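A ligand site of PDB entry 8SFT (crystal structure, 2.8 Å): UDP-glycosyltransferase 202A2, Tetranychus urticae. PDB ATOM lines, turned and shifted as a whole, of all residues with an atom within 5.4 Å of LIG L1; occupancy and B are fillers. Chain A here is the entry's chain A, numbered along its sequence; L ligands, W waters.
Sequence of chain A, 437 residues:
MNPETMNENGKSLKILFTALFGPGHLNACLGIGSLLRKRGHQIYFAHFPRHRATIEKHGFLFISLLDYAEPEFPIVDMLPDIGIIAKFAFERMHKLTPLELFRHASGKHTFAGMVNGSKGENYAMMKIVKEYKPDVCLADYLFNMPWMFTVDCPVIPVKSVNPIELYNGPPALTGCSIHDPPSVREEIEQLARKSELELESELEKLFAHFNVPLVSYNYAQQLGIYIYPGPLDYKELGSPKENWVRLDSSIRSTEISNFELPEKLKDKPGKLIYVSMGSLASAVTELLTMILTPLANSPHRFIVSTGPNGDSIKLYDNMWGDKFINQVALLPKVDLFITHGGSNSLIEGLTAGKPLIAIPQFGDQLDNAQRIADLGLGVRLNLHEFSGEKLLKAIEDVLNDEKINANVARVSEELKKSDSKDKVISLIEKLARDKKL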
ATOM      1  N   GLY A  22     -18.014  22.683   5.537  1.00  0.00           N
ATOM      2  CA  GLY A  22     -17.677  22.658   4.098  1.00  0.00           C
ATOM      3  C   GLY A  22     -16.731  21.510   3.773  1.00  0.00           C
ATOM      4  O   GLY A  22     -15.642  21.418   4.335  1.00  0.00           O
ATOM      5  N   PRO A  23     -17.140  20.595   2.857  1.00  0.00           N
ATOM      6  CA  PRO A  23     -16.258  19.551   2.335  1.00  0.00           C
ATOM      7  C   PRO A  23     -14.869  20.022   1.863  1.00  0.00           C
ATOM      8  O   PRO A  23     -13.929  19.255   1.966  1.00  0.00           O
ATOM      9  CB  PRO A  23     -17.071  18.991   1.174  1.00  0.00           C
ATOM     10  CG  PRO A  23     -18.486  19.108   1.673  1.00  0.00           C
ATOM     11  CD  PRO A  23     -18.532  20.439   2.380  1.00  0.00           C
ATOM     12  N   GLY A  24     -14.771  21.253   1.358  1.00  0.00           N
ATOM     13  CA  GLY A  24     -13.474  21.847   0.971  1.00  0.00           C
ATOM     14  C   GLY A  24     -12.514  21.891   2.138  1.00  0.00           C
ATOM     15  O   GLY A  24     -11.333  21.535   1.961  1.00  0.00           O
ATOM     16  N   HIS A  25     -12.995  22.276   3.320  1.00  0.00           N
ATOM     17  CA  HIS A  25     -12.174  22.399   4.543  1.00  0.00           C
ATOM     18  C   HIS A  25     -11.801  21.002   5.051  1.00  0.00           C
ATOM     19  O   HIS A  25     -10.617  20.782   5.387  1.00  0.00           O
ATOM     20  CB  HIS A  25     -12.916  23.301   5.537  1.00  0.00           C
ATOM     21  CG  HIS A  25     -13.178  24.642   4.961  1.00  0.00           C
ATOM     22  ND1 HIS A  25     -12.310  25.699   5.120  1.00  0.00           N
ATOM     23  CD2 HIS A  25     -14.184  25.101   4.172  1.00  0.00           C
ATOM     24  CE1 HIS A  25     -12.784  26.752   4.495  1.00  0.00           C
ATOM     25  NE2 HIS A  25     -13.927  26.411   3.872  1.00  0.00           N
ATOM     26  N   ASN A  27     -11.610  18.263   3.256  1.00  0.00           N
ATOM     27  CA  ASN A  27     -10.812  17.516   2.254  1.00  0.00           C
ATOM     28  C   ASN A  27      -9.364  17.924   2.409  1.00  0.00           C
ATOM     29  O   ASN A  27      -8.502  17.033   2.412  1.00  0.00           O
ATOM     30  CB  ASN A  27     -11.333  17.700   0.814  1.00  0.00           C
ATOM     31  CG  ASN A  27     -12.555  16.858   0.514  1.00  0.00           C
ATOM     32  OD1 ASN A  27     -12.966  16.030   1.326  1.00  0.00           O
ATOM     33  ND2 ASN A  27     -13.173  17.047  -0.634  1.00  0.00           N
ATOM     34  N   ARG A 252      -6.446  14.382  -0.930  1.00  0.00           N
ATOM     35  CA  ARG A 252      -6.877  13.118  -0.253  1.00  0.00           C
ATOM     36  C   ARG A 252      -6.612  11.906  -1.150  1.00  0.00           C
ATOM     37  O   ARG A 252      -6.543  12.051  -2.392  1.00  0.00           O
ATOM     38  CB  ARG A 252      -8.363  13.222   0.139  1.00  0.00           C
ATOM     39  CG  ARG A 252      -9.305  13.450  -1.032  1.00  0.00           C
ATOM     40  CD  ARG A 252     -10.644  14.032  -0.579  1.00  0.00           C
ATOM     41  NE  ARG A 252     -11.585  14.189  -1.691  1.00  0.00           N
ATOM     42  CZ  ARG A 252     -11.484  15.111  -2.654  1.00  0.00           C
ATOM     43  NH1 ARG A 252     -12.395  15.150  -3.616  1.00  0.00           N
ATOM     44  NH2 ARG A 252     -10.493  15.983  -2.656  1.00  0.00           N
ATOM     45  N   TYR A 274     -15.321  18.989 -17.683  1.00  0.00           N
ATOM     46  CA  TYR A 274     -15.926  18.834 -16.338  1.00  0.00           C
ATOM     47  C   TYR A 274     -16.530  20.172 -15.904  1.00  0.00           C
ATOM     48  O   TYR A 274     -15.871  21.213 -16.061  1.00  0.00           O
ATOM     49  CB  TYR A 274     -14.865  18.339 -15.368  1.00  0.00           C
ATOM     50  CG  TYR A 274     -15.346  18.109 -13.966  1.00  0.00           C
ATOM     51  CD1 TYR A 274     -16.529  17.431 -13.708  1.00  0.00           C
ATOM     52  CD2 TYR A 274     -14.606  18.541 -12.882  1.00  0.00           C
ATOM     53  CE1 TYR A 274     -16.966  17.206 -12.406  1.00  0.00           C
ATOM     54  CE2 TYR A 274     -15.014  18.314 -11.577  1.00  0.00           C
ATOM     55  CZ  TYR A 274     -16.189  17.623 -11.336  1.00  0.00           C
ATOM     56  OH  TYR A 274     -16.615  17.398 -10.053  1.00  0.00           O
ATOM     57  N   SER A 276     -18.334  21.527 -12.398  1.00  0.00           N
ATOM     58  CA  SER A 276     -18.821  21.548 -11.000  1.00  0.00           C
ATOM     59  C   SER A 276     -18.757  22.979 -10.451  1.00  0.00           C
ATOM     60  O   SER A 276     -17.817  23.709 -10.807  1.00  0.00           O
ATOM     61  CB  SER A 276     -18.049  20.606 -10.127  1.00  0.00           C
ATOM     62  OG  SER A 276     -18.516  20.662  -8.789  1.00  0.00           O
ATOM     63  N   MET A 277     -19.718  23.332  -9.610  1.00  0.00           N
ATOM     64  CA  MET A 277     -19.752  24.654  -8.933  1.00  0.00           C
ATOM     65  C   MET A 277     -19.462  24.457  -7.441  1.00  0.00           C
ATOM     66  O   MET A 277     -19.689  25.391  -6.669  1.00  0.00           O
ATOM     67  CB  MET A 277     -21.124  25.315  -9.100  1.00  0.00           C
ATOM     68  CG  MET A 277     -21.312  25.973 -10.459  1.00  0.00           C
ATOM     69  SD  MET A 277     -20.108  27.275 -10.818  1.00  0.00           S
ATOM     70  CE  MET A 277     -19.133  26.471 -12.088  1.00  0.00           C
ATOM     71  N   GLY A 278     -18.962  23.271  -7.069  1.00  0.00           N
ATOM     72  CA  GLY A 278     -18.342  23.047  -5.751  1.00  0.00           C
ATOM     73  C   GLY A 278     -19.228  22.264  -4.798  1.00  0.00           C
ATOM     74  O   GLY A 278     -20.104  21.525  -5.277  1.00  0.00           O
ATOM     75  N   SER A 279     -18.979  22.429  -3.494  1.00  0.00           N
ATOM     76  CA  SER A 279     -19.681  21.677  -2.426  1.00  0.00           C
ATOM     77  C   SER A 279     -20.910  22.453  -1.957  1.00  0.00           C
ATOM     78  O   SER A 279     -21.805  21.835  -1.336  1.00  0.00           O
ATOM     79  CB  SER A 279     -18.739  21.389  -1.287  1.00  0.00           C
ATOM     80  OG  SER A 279     -18.043  22.561  -0.903  1.00  0.00           O
ATOM     81  N   LEU A 280     -20.956  23.747  -2.256  1.00  0.00           N
ATOM     82  CA  LEU A 280     -21.844  24.737  -1.595  1.00  0.00           C
ATOM     83  C   LEU A 280     -22.720  25.413  -2.650  1.00  0.00           C
ATOM     84  O   LEU A 280     -23.959  25.274  -2.553  1.00  0.00           O
ATOM     85  CB  LEU A 280     -20.976  25.752  -0.841  1.00  0.00           C
ATOM     86  CG  LEU A 280     -19.940  25.158   0.124  1.00  0.00           C
ATOM     87  CD1 LEU A 280     -19.137  26.252   0.790  1.00  0.00           C
ATOM     88  CD2 LEU A 280     -20.593  24.257   1.169  1.00  0.00           C
ATOM     89  N   ALA A 281     -22.098  26.089  -3.620  1.00  0.00           N
ATOM     90  CA  ALA A 281     -22.802  26.853  -4.673  1.00  0.00           C
ATOM     91  C   ALA A 281     -23.621  25.904  -5.554  1.00  0.00           C
ATOM     92  O   ALA A 281     -24.584  26.373  -6.184  1.00  0.00           O
ATOM     93  CB  ALA A 281     -21.817  27.656  -5.475  1.00  0.00           C
ATOM     94  N   SER A 305     -21.157  17.712 -12.191  1.00  0.00           N
ATOM     95  CA  SER A 305     -21.541  17.560 -10.771  1.00  0.00           C
ATOM     96  C   SER A 305     -22.804  18.404 -10.591  1.00  0.00           C
ATOM     97  O   SER A 305     -22.715  19.628 -10.759  1.00  0.00           O
ATOM     98  CB  SER A 305     -20.418  17.963  -9.896  1.00  0.00           C
ATOM     99  OG  SER A 305     -20.715  17.763  -8.543  1.00  0.00           O
ATOM    100  N   LYS A 323     -25.179  13.754  -8.720  1.00  0.00           N
ATOM    101  CA  LYS A 323     -25.174  14.725  -7.604  1.00  0.00           C
ATOM    102  C   LYS A 323     -23.735  14.896  -7.128  1.00  0.00           C
ATOM    103  O   LYS A 323     -23.331  16.034  -6.900  1.00  0.00           O
ATOM    104  CB  LYS A 323     -26.126  14.274  -6.490  1.00  0.00           C
ATOM    105  CG  LYS A 323     -27.556  14.048  -6.923  1.00  0.00           C
ATOM    106  CD  LYS A 323     -28.564  14.081  -5.791  1.00  0.00           C
ATOM    107  CE  LYS A 323     -28.452  12.890  -4.887  1.00  0.00           C
ATOM    108  NZ  LYS A 323     -29.254  13.085  -3.657  1.00  0.00           N
ATOM    109  N   PHE A 324     -23.005  13.790  -6.977  1.00  0.00           N
ATOM    110  CA  PHE A 324     -21.602  13.716  -6.535  1.00  0.00           C
ATOM    111  C   PHE A 324     -20.797  12.934  -7.590  1.00  0.00           C
ATOM    112  O   PHE A 324     -21.280  11.919  -8.093  1.00  0.00           O
ATOM    113  CB  PHE A 324     -21.556  13.094  -5.148  1.00  0.00           C
ATOM    114  CG  PHE A 324     -20.210  13.115  -4.468  1.00  0.00           C
ATOM    115  CD1 PHE A 324     -19.735  14.281  -3.864  1.00  0.00           C
ATOM    116  CD2 PHE A 324     -19.408  11.963  -4.435  1.00  0.00           C
ATOM    117  CE1 PHE A 324     -18.480  14.293  -3.267  1.00  0.00           C
ATOM    118  CE2 PHE A 324     -18.166  11.982  -3.825  1.00  0.00           C
ATOM    119  CZ  PHE A 324     -17.696  13.151  -3.245  1.00  0.00           C
ATOM    120  N   ILE A 325     -19.595  13.426  -7.915  1.00  0.00           N
ATOM    121  CA  ILE A 325     -18.670  12.840  -8.926  1.00  0.00           C
ATOM    122  C   ILE A 325     -17.377  12.542  -8.190  1.00  0.00           C
ATOM    123  O   ILE A 325     -17.050  13.344  -7.289  1.00  0.00           O
ATOM    124  CB  ILE A 325     -18.432  13.857 -10.061  1.00  0.00           C
ATOM    125  CG1 ILE A 325     -19.699  14.167 -10.855  1.00  0.00           C
ATOM    126  CG2 ILE A 325     -17.321  13.396 -10.977  1.00  0.00           C
ATOM    127  CD1 ILE A 325     -20.054  13.088 -11.827  1.00  0.00           C
ATOM    128  N   ASN A 326     -16.671  11.463  -8.522  1.00  0.00           N
ATOM    129  CA  ASN A 326     -15.310  11.261  -7.991  1.00  0.00           C
ATOM    130  C   ASN A 326     -14.380  12.175  -8.822  1.00  0.00           C
ATOM    131  O   ASN A 326     -13.811  11.726  -9.833  1.00  0.00           O
ATOM    132  CB  ASN A 326     -14.893   9.793  -7.930  1.00  0.00           C
ATOM    133  CG  ASN A 326     -13.491   9.619  -7.384  1.00  0.00           C
ATOM    134  OD1 ASN A 326     -12.810  10.578  -6.994  1.00  0.00           O
ATOM    135  ND2 ASN A 326     -13.045   8.374  -7.367  1.00  0.00           N
ATOM    136  N   GLN A 327     -14.246  13.418  -8.345  1.00  0.00           N
ATOM    137  CA  GLN A 327     -13.562  14.558  -9.002  1.00  0.00           C
ATOM    138  C   GLN A 327     -12.076  14.255  -9.215  1.00  0.00           C
ATOM    139  O   GLN A 327     -11.565  14.501 -10.329  1.00  0.00           O
ATOM    140  CB  GLN A 327     -13.833  15.817  -8.188  1.00  0.00           C
ATOM    141  CG  GLN A 327     -13.106  17.041  -8.727  1.00  0.00           C
ATOM    142  CD  GLN A 327     -13.699  18.353  -8.250  1.00  0.00           C
ATOM    143  OE1 GLN A 327     -14.899  18.547  -8.281  1.00  0.00           O
ATOM    144  NE2 GLN A 327     -12.838  19.258  -7.801  1.00  0.00           N
ATOM    145  N   VAL A 328     -11.413  13.679  -8.235  1.00  0.00           N
ATOM    146  CA  VAL A 328      -9.939  13.449  -8.323  1.00  0.00           C
ATOM    147  C   VAL A 328      -9.656  12.368  -9.372  1.00  0.00           C
ATOM    148  O   VAL A 328      -8.710  12.528 -10.163  1.00  0.00           O
ATOM    149  CB  VAL A 328      -9.322  13.090  -6.966  1.00  0.00           C
ATOM    150  CG1 VAL A 328      -7.854  12.793  -7.137  1.00  0.00           C
ATOM    151  CG2 VAL A 328      -9.556  14.158  -5.902  1.00  0.00           C
ATOM    152  N   HIS A 340     -15.919  27.082 -10.006  1.00  0.00           N
ATOM    153  CA  HIS A 340     -16.498  28.249  -9.284  1.00  0.00           C
ATOM    154  C   HIS A 340     -15.384  29.078  -8.646  1.00  0.00           C
ATOM    155  O   HIS A 340     -15.620  30.214  -8.211  1.00  0.00           O
ATOM    156  CB  HIS A 340     -17.503  27.766  -8.230  1.00  0.00           C
ATOM    157  CG  HIS A 340     -16.876  27.003  -7.104  1.00  0.00           C
ATOM    158  ND1 HIS A 340     -16.221  25.811  -7.284  1.00  0.00           N
ATOM    159  CD2 HIS A 340     -16.833  27.258  -5.797  1.00  0.00           C
ATOM    160  CE1 HIS A 340     -15.783  25.367  -6.116  1.00  0.00           C
ATOM    161  NE2 HIS A 340     -16.138  26.242  -5.197  1.00  0.00           N
ATOM    162  N   GLY A 342     -13.181  27.489  -6.303  1.00  0.00           N
ATOM    163  CA  GLY A 342     -12.801  26.855  -5.046  1.00  0.00           C
ATOM    164  C   GLY A 342     -11.350  26.435  -5.102  1.00  0.00           C
ATOM    165  O   GLY A 342     -10.850  26.099  -6.193  1.00  0.00           O
ATOM    166  N   SER A 343     -10.673  26.460  -3.959  1.00  0.00           N
ATOM    167  CA  SER A 343      -9.219  26.252  -3.854  1.00  0.00           C
ATOM    168  C   SER A 343      -8.913  24.780  -4.115  1.00  0.00           C
ATOM    169  O   SER A 343      -7.976  24.505  -4.865  1.00  0.00           O
ATOM    170  CB  SER A 343      -8.707  26.703  -2.507  1.00  0.00           C
ATOM    171  OG  SER A 343      -8.552  28.101  -2.486  1.00  0.00           O
ATOM    172  N   ASN A 344      -9.661  23.855  -3.509  1.00  0.00           N
ATOM    173  CA  ASN A 344      -9.380  22.411  -3.701  1.00  0.00           C
ATOM    174  C   ASN A 344      -9.536  22.054  -5.180  1.00  0.00           C
ATOM    175  O   ASN A 344      -8.717  21.296  -5.693  1.00  0.00           O
ATOM    176  CB  ASN A 344     -10.288  21.546  -2.857  1.00  0.00           C
ATOM    177  CG  ASN A 344      -9.970  21.706  -1.389  1.00  0.00           C
ATOM    178  OD1 ASN A 344      -8.997  21.124  -0.895  1.00  0.00           O
ATOM    179  ND2 ASN A 344     -10.795  22.468  -0.704  1.00  0.00           N
ATOM    180  N   SER A 345     -10.565  22.577  -5.834  1.00  0.00           N
ATOM    181  CA  SER A 345     -10.828  22.344  -7.279  1.00  0.00           C
ATOM    182  C   SER A 345      -9.696  22.914  -8.138  1.00  0.00           C
ATOM    183  O   SER A 345      -9.312  22.281  -9.128  1.00  0.00           O
ATOM    184  CB  SER A 345     -12.158  22.924  -7.680  1.00  0.00           C
ATOM    185  OG  SER A 345     -13.211  22.262  -7.004  1.00  0.00           O
ATOM    186  N   LEU A 346      -9.204  24.101  -7.786  1.00  0.00           N
ATOM    187  CA  LEU A 346      -8.073  24.766  -8.471  1.00  0.00           C
ATOM    188  C   LEU A 346      -6.865  23.829  -8.401  1.00  0.00           C
ATOM    189  O   LEU A 346      -6.300  23.489  -9.446  1.00  0.00           O
ATOM    190  CB  LEU A 346      -7.826  26.095  -7.750  1.00  0.00           C
ATOM    191  CG  LEU A 346      -6.610  26.901  -8.155  1.00  0.00           C
ATOM    192  CD1 LEU A 346      -6.715  27.285  -9.621  1.00  0.00           C
ATOM    193  CD2 LEU A 346      -6.521  28.134  -7.301  1.00  0.00           C
ATOM    194  N   GLU A 348      -6.643  20.559  -7.475  1.00  0.00           N
ATOM    195  CA  GLU A 348      -6.975  19.253  -8.096  1.00  0.00           C
ATOM    196  C   GLU A 348      -6.838  19.367  -9.617  1.00  0.00           C
ATOM    197  O   GLU A 348      -6.197  18.499 -10.258  1.00  0.00           O
ATOM    198  CB  GLU A 348      -8.379  18.833  -7.654  1.00  0.00           C
ATOM    199  CG  GLU A 348      -8.402  18.303  -6.221  1.00  0.00           C
ATOM    200  CD  GLU A 348      -9.748  18.292  -5.521  1.00  0.00           C
ATOM    201  OE1 GLU A 348     -10.789  18.383  -6.206  1.00  0.00           O
ATOM    202  OE2 GLU A 348      -9.749  18.189  -4.305  1.00  0.00           O
ATOM    203  N   GLN A 365     -13.266  32.689  -3.761  1.00  0.00           N
ATOM    204  CA  GLN A 365     -13.465  32.268  -5.172  1.00  0.00           C
ATOM    205  C   GLN A 365     -13.112  33.427  -6.124  1.00  0.00           C
ATOM    206  O   GLN A 365     -12.511  33.119  -7.178  1.00  0.00           O
ATOM    207  CB  GLN A 365     -14.887  31.784  -5.400  1.00  0.00           C
ATOM    208  CG  GLN A 365     -15.260  30.553  -4.576  1.00  0.00           C
ATOM    209  CD  GLN A 365     -16.748  30.429  -4.466  1.00  0.00           C
ATOM    210  OE1 GLN A 365     -17.493  30.950  -5.281  1.00  0.00           O
ATOM    211  NE2 GLN A 365     -17.193  29.743  -3.449  1.00  0.00           N
HETATM  212  N1  LIG L   1     -15.947  17.463  -4.863  1.00  0.00           N
HETATM  213  C1  LIG L   1     -15.987  16.114  -5.187  1.00  0.00           C
HETATM  214  N2  LIG L   1     -17.007  15.758  -6.033  1.00  0.00           N
HETATM  215  C2  LIG L   1     -17.958  16.594  -6.582  1.00  0.00           C
HETATM  216  C3  LIG L   1     -17.848  17.962  -6.204  1.00  0.00           C
HETATM  217  C4  LIG L   1     -16.859  18.347  -5.376  1.00  0.00           C
HETATM  218  O1  LIG L   1     -15.186  15.298  -4.743  1.00  0.00           O
HETATM  219  O2  LIG L   1     -18.808  16.110  -7.339  1.00  0.00           O
HETATM  220  C5  LIG L   1     -14.868  17.895  -3.959  1.00  0.00           C
HETATM  221  C6  LIG L   1     -13.631  18.386  -4.699  1.00  0.00           C
HETATM  222  O3  LIG L   1     -12.812  17.267  -5.009  1.00  0.00           O
HETATM  223  C7  LIG L   1     -13.005  19.322  -3.659  1.00  0.00           C
HETATM  224  C8  LIG L   1     -14.218  19.891  -2.906  1.00  0.00           C
HETATM  225  O4  LIG L   1     -15.329  18.998  -3.211  1.00  0.00           O
HETATM  226  O5  LIG L   1     -12.139  18.619  -2.763  1.00  0.00           O
HETATM  227  C9  LIG L   1     -14.594  21.304  -3.263  1.00  0.00           C
HETATM  228  O6  LIG L   1     -13.633  22.212  -2.668  1.00  0.00           O
HETATM  229  P1  LIG L   1     -13.504  23.695  -3.263  1.00  0.00           P
HETATM  230  O7  LIG L   1     -13.060  23.614  -4.694  1.00  0.00           O
HETATM  231  O8  LIG L   1     -12.701  24.536  -2.339  1.00  0.00           O
HETATM  232  O9  LIG L   1     -15.030  24.179  -3.232  1.00  0.00           O
HETATM  233  P2  LIG L   1     -16.002  24.740  -2.082  1.00  0.00           P
HETATM  234  O10 LIG L   1     -17.397  24.653  -2.635  1.00  0.00           O
HETATM  235  O11 LIG L   1     -15.563  26.159  -1.826  1.00  0.00           O
HETATM  236  O12 LIG L   1     -15.798  23.849  -0.882  1.00  0.00           O
HETATM  237  C1  LG2 L   2     -23.040  31.361   6.275  1.00  0.00           C
HETATM  238  C2  LG2 L   2     -22.269  32.222   5.535  1.00  0.00           C
HETATM  239  C3  LG2 L   2     -21.124  31.758   4.856  1.00  0.00           C
HETATM  240  C4  LG2 L   2     -20.807  30.402   4.981  1.00  0.00           C
HETATM  241  C5  LG2 L   2     -21.550  29.509   5.723  1.00  0.00           C
HETATM  242  C6  LG2 L   2     -22.677  30.007   6.372  1.00  0.00           C
HETATM  243  C7  LG2 L   2     -20.267  32.617   4.054  1.00  0.00           C
HETATM  244  C8  LG2 L   2     -19.132  31.984   3.426  1.00  0.00           C
HETATM  245  C9  LG2 L   2     -18.882  30.658   3.589  1.00  0.00           C
HETATM  246  C10 LG2 L   2     -17.749  29.920   3.002  1.00  0.00           C
HETATM  247  C11 LG2 L   2     -16.737  30.582   2.296  1.00  0.00           C
HETATM  248  C12 LG2 L   2     -15.672  29.892   1.767  1.00  0.00           C
HETATM  249  C13 LG2 L   2     -15.594  28.514   1.923  1.00  0.00           C
HETATM  250  C14 LG2 L   2     -16.583  27.845   2.628  1.00  0.00           C
HETATM  251  C15 LG2 L   2     -17.642  28.541   3.160  1.00  0.00           C
HETATM  252  O1  LG2 L   2     -19.710  29.888   4.357  1.00  0.00           O
HETATM  253  O2  LG2 L   2     -20.483  33.842   3.891  1.00  0.00           O
HETATM  254  O3  LG2 L   2     -14.528  27.825   1.394  1.00  0.00           O
HETATM  255  O4  LG2 L   2     -18.323  32.784   2.668  1.00  0.00           O
HETATM  256  O5  LG2 L   2     -23.448  29.155   7.122  1.00  0.00           O
HETATM  257  O6  LG2 L   2     -22.592  33.544   5.422  1.00  0.00           O
HETATM  258  O   HOH W   1     -15.413  28.636  -2.016  1.00  0.00           O
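NH1 of Arg 252 is in hydrogen-bond range of O3 of LIG L1 (2.6 Å).
N of Ser 279 lies within hydrogen-bond range of O10 of LIG L1.
OG of Ser 279 lies within hydrogen-bond range of O12 of LIG L1 (2.6 Å).
The side-chain carboxylate (OE1) of Glu 348 lies within hydrogen-bond range of an oxygen (O3) of LIG L1 (2.6 Å).
O7 of LIG L1 is in hydrogen-bond range of N of Ser 345, at 2.9 Å.
The side-chain hydroxyl (OG) of Ser 345 sits at hydrogen-bond distance from an oxygen (O7) of LIG L1.
An oxygen (O2) of LIG L1 is in hydrogen-bond range of the backbone NH of Ile 325, at 2.9 Å.
O of Ile 325 sits at hydrogen-bond distance from N2 of LIG L1, 2.7 Å away.
The side-chain hydroxyl (OG) of Ser 305 is in hydrogen-bond range of an oxygen (O2) of LIG L1.
O5 of LIG L1 is in hydrogen-bond range of ND2 of Asn 27.
NE2 of His 340 is in hydrogen-bond range of O9 of LIG L1 (3.1 Å).
O8 of LIG L1 lies within hydrogen-bond range of N of Ser 343 (3.2 Å).
N of Asn 344 sits at hydrogen-bond distance from O8 of LIG L1 (3.3 Å).
ND2 of Asn 344 is in hydrogen-bond range of O8 of LIG L1 (3.3 Å).
The side-chain amide nitrogen (NE2) of Gln 327 sits close to an oxygen (O3) of LIG L1, at 3.4 Å.
NE2 of His 25 is in hydrogen-bond range of O3 of LG2 L2 (2.9 Å).
Residues that only touch LIG L1: Gly 24 (3.6 Å), Tyr 274 (3.7 Å), Ser 276 (3.8 Å), Gly 278 (3.6 Å), Leu 280 (3.7 Å), Phe 324 (3.5 Å) and Gly 342 (3.3 Å).
The nearest printed residue that does not touch LIG L1 is Gln 365 (4.3 Å).
Water W1 lies within hydrogen-bond range of an oxygen (O11) of LIG L1 (2.5 Å) and the side-chain amide nitrogen (NE2) of Gln 365 (2.5 Å).
The side-chain amide nitrogen of Asn 27 sits close to the guanidinium group of Arg 252 (3.4 Å).
NE2 of Gln 327 sits at hydrogen-bond distance from OE1 of Glu 348, at 2.7 Å.
The side-chain amide nitrogen (NE2) of Gln 327 lies within hydrogen-bond range of the side-chain hydroxyl (OG) of Ser 345, at 3.1 Å.
The backbone carbonyl oxygen (O) of Pro 23 lies close to the side-chain amide oxygen (OD1) of Asn 27.
NE2 of His 340 lies close to N of Gly 342, 3.4 Å away.
The side-chain amide nitrogen (ND2) of Asn 344 sits at hydrogen-bond distance from the backbone carbonyl oxygen (O) of Gly 24 (2.9 Å).
OH of Tyr 274 lies within hydrogen-bond range of OE1 of Gln 327 (2.7 Å).
The backbone NH (N) of Gly 278 lies within hydrogen-bond range of the side-chain hydroxyl (OG) of Ser 276 (3.2 Å).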
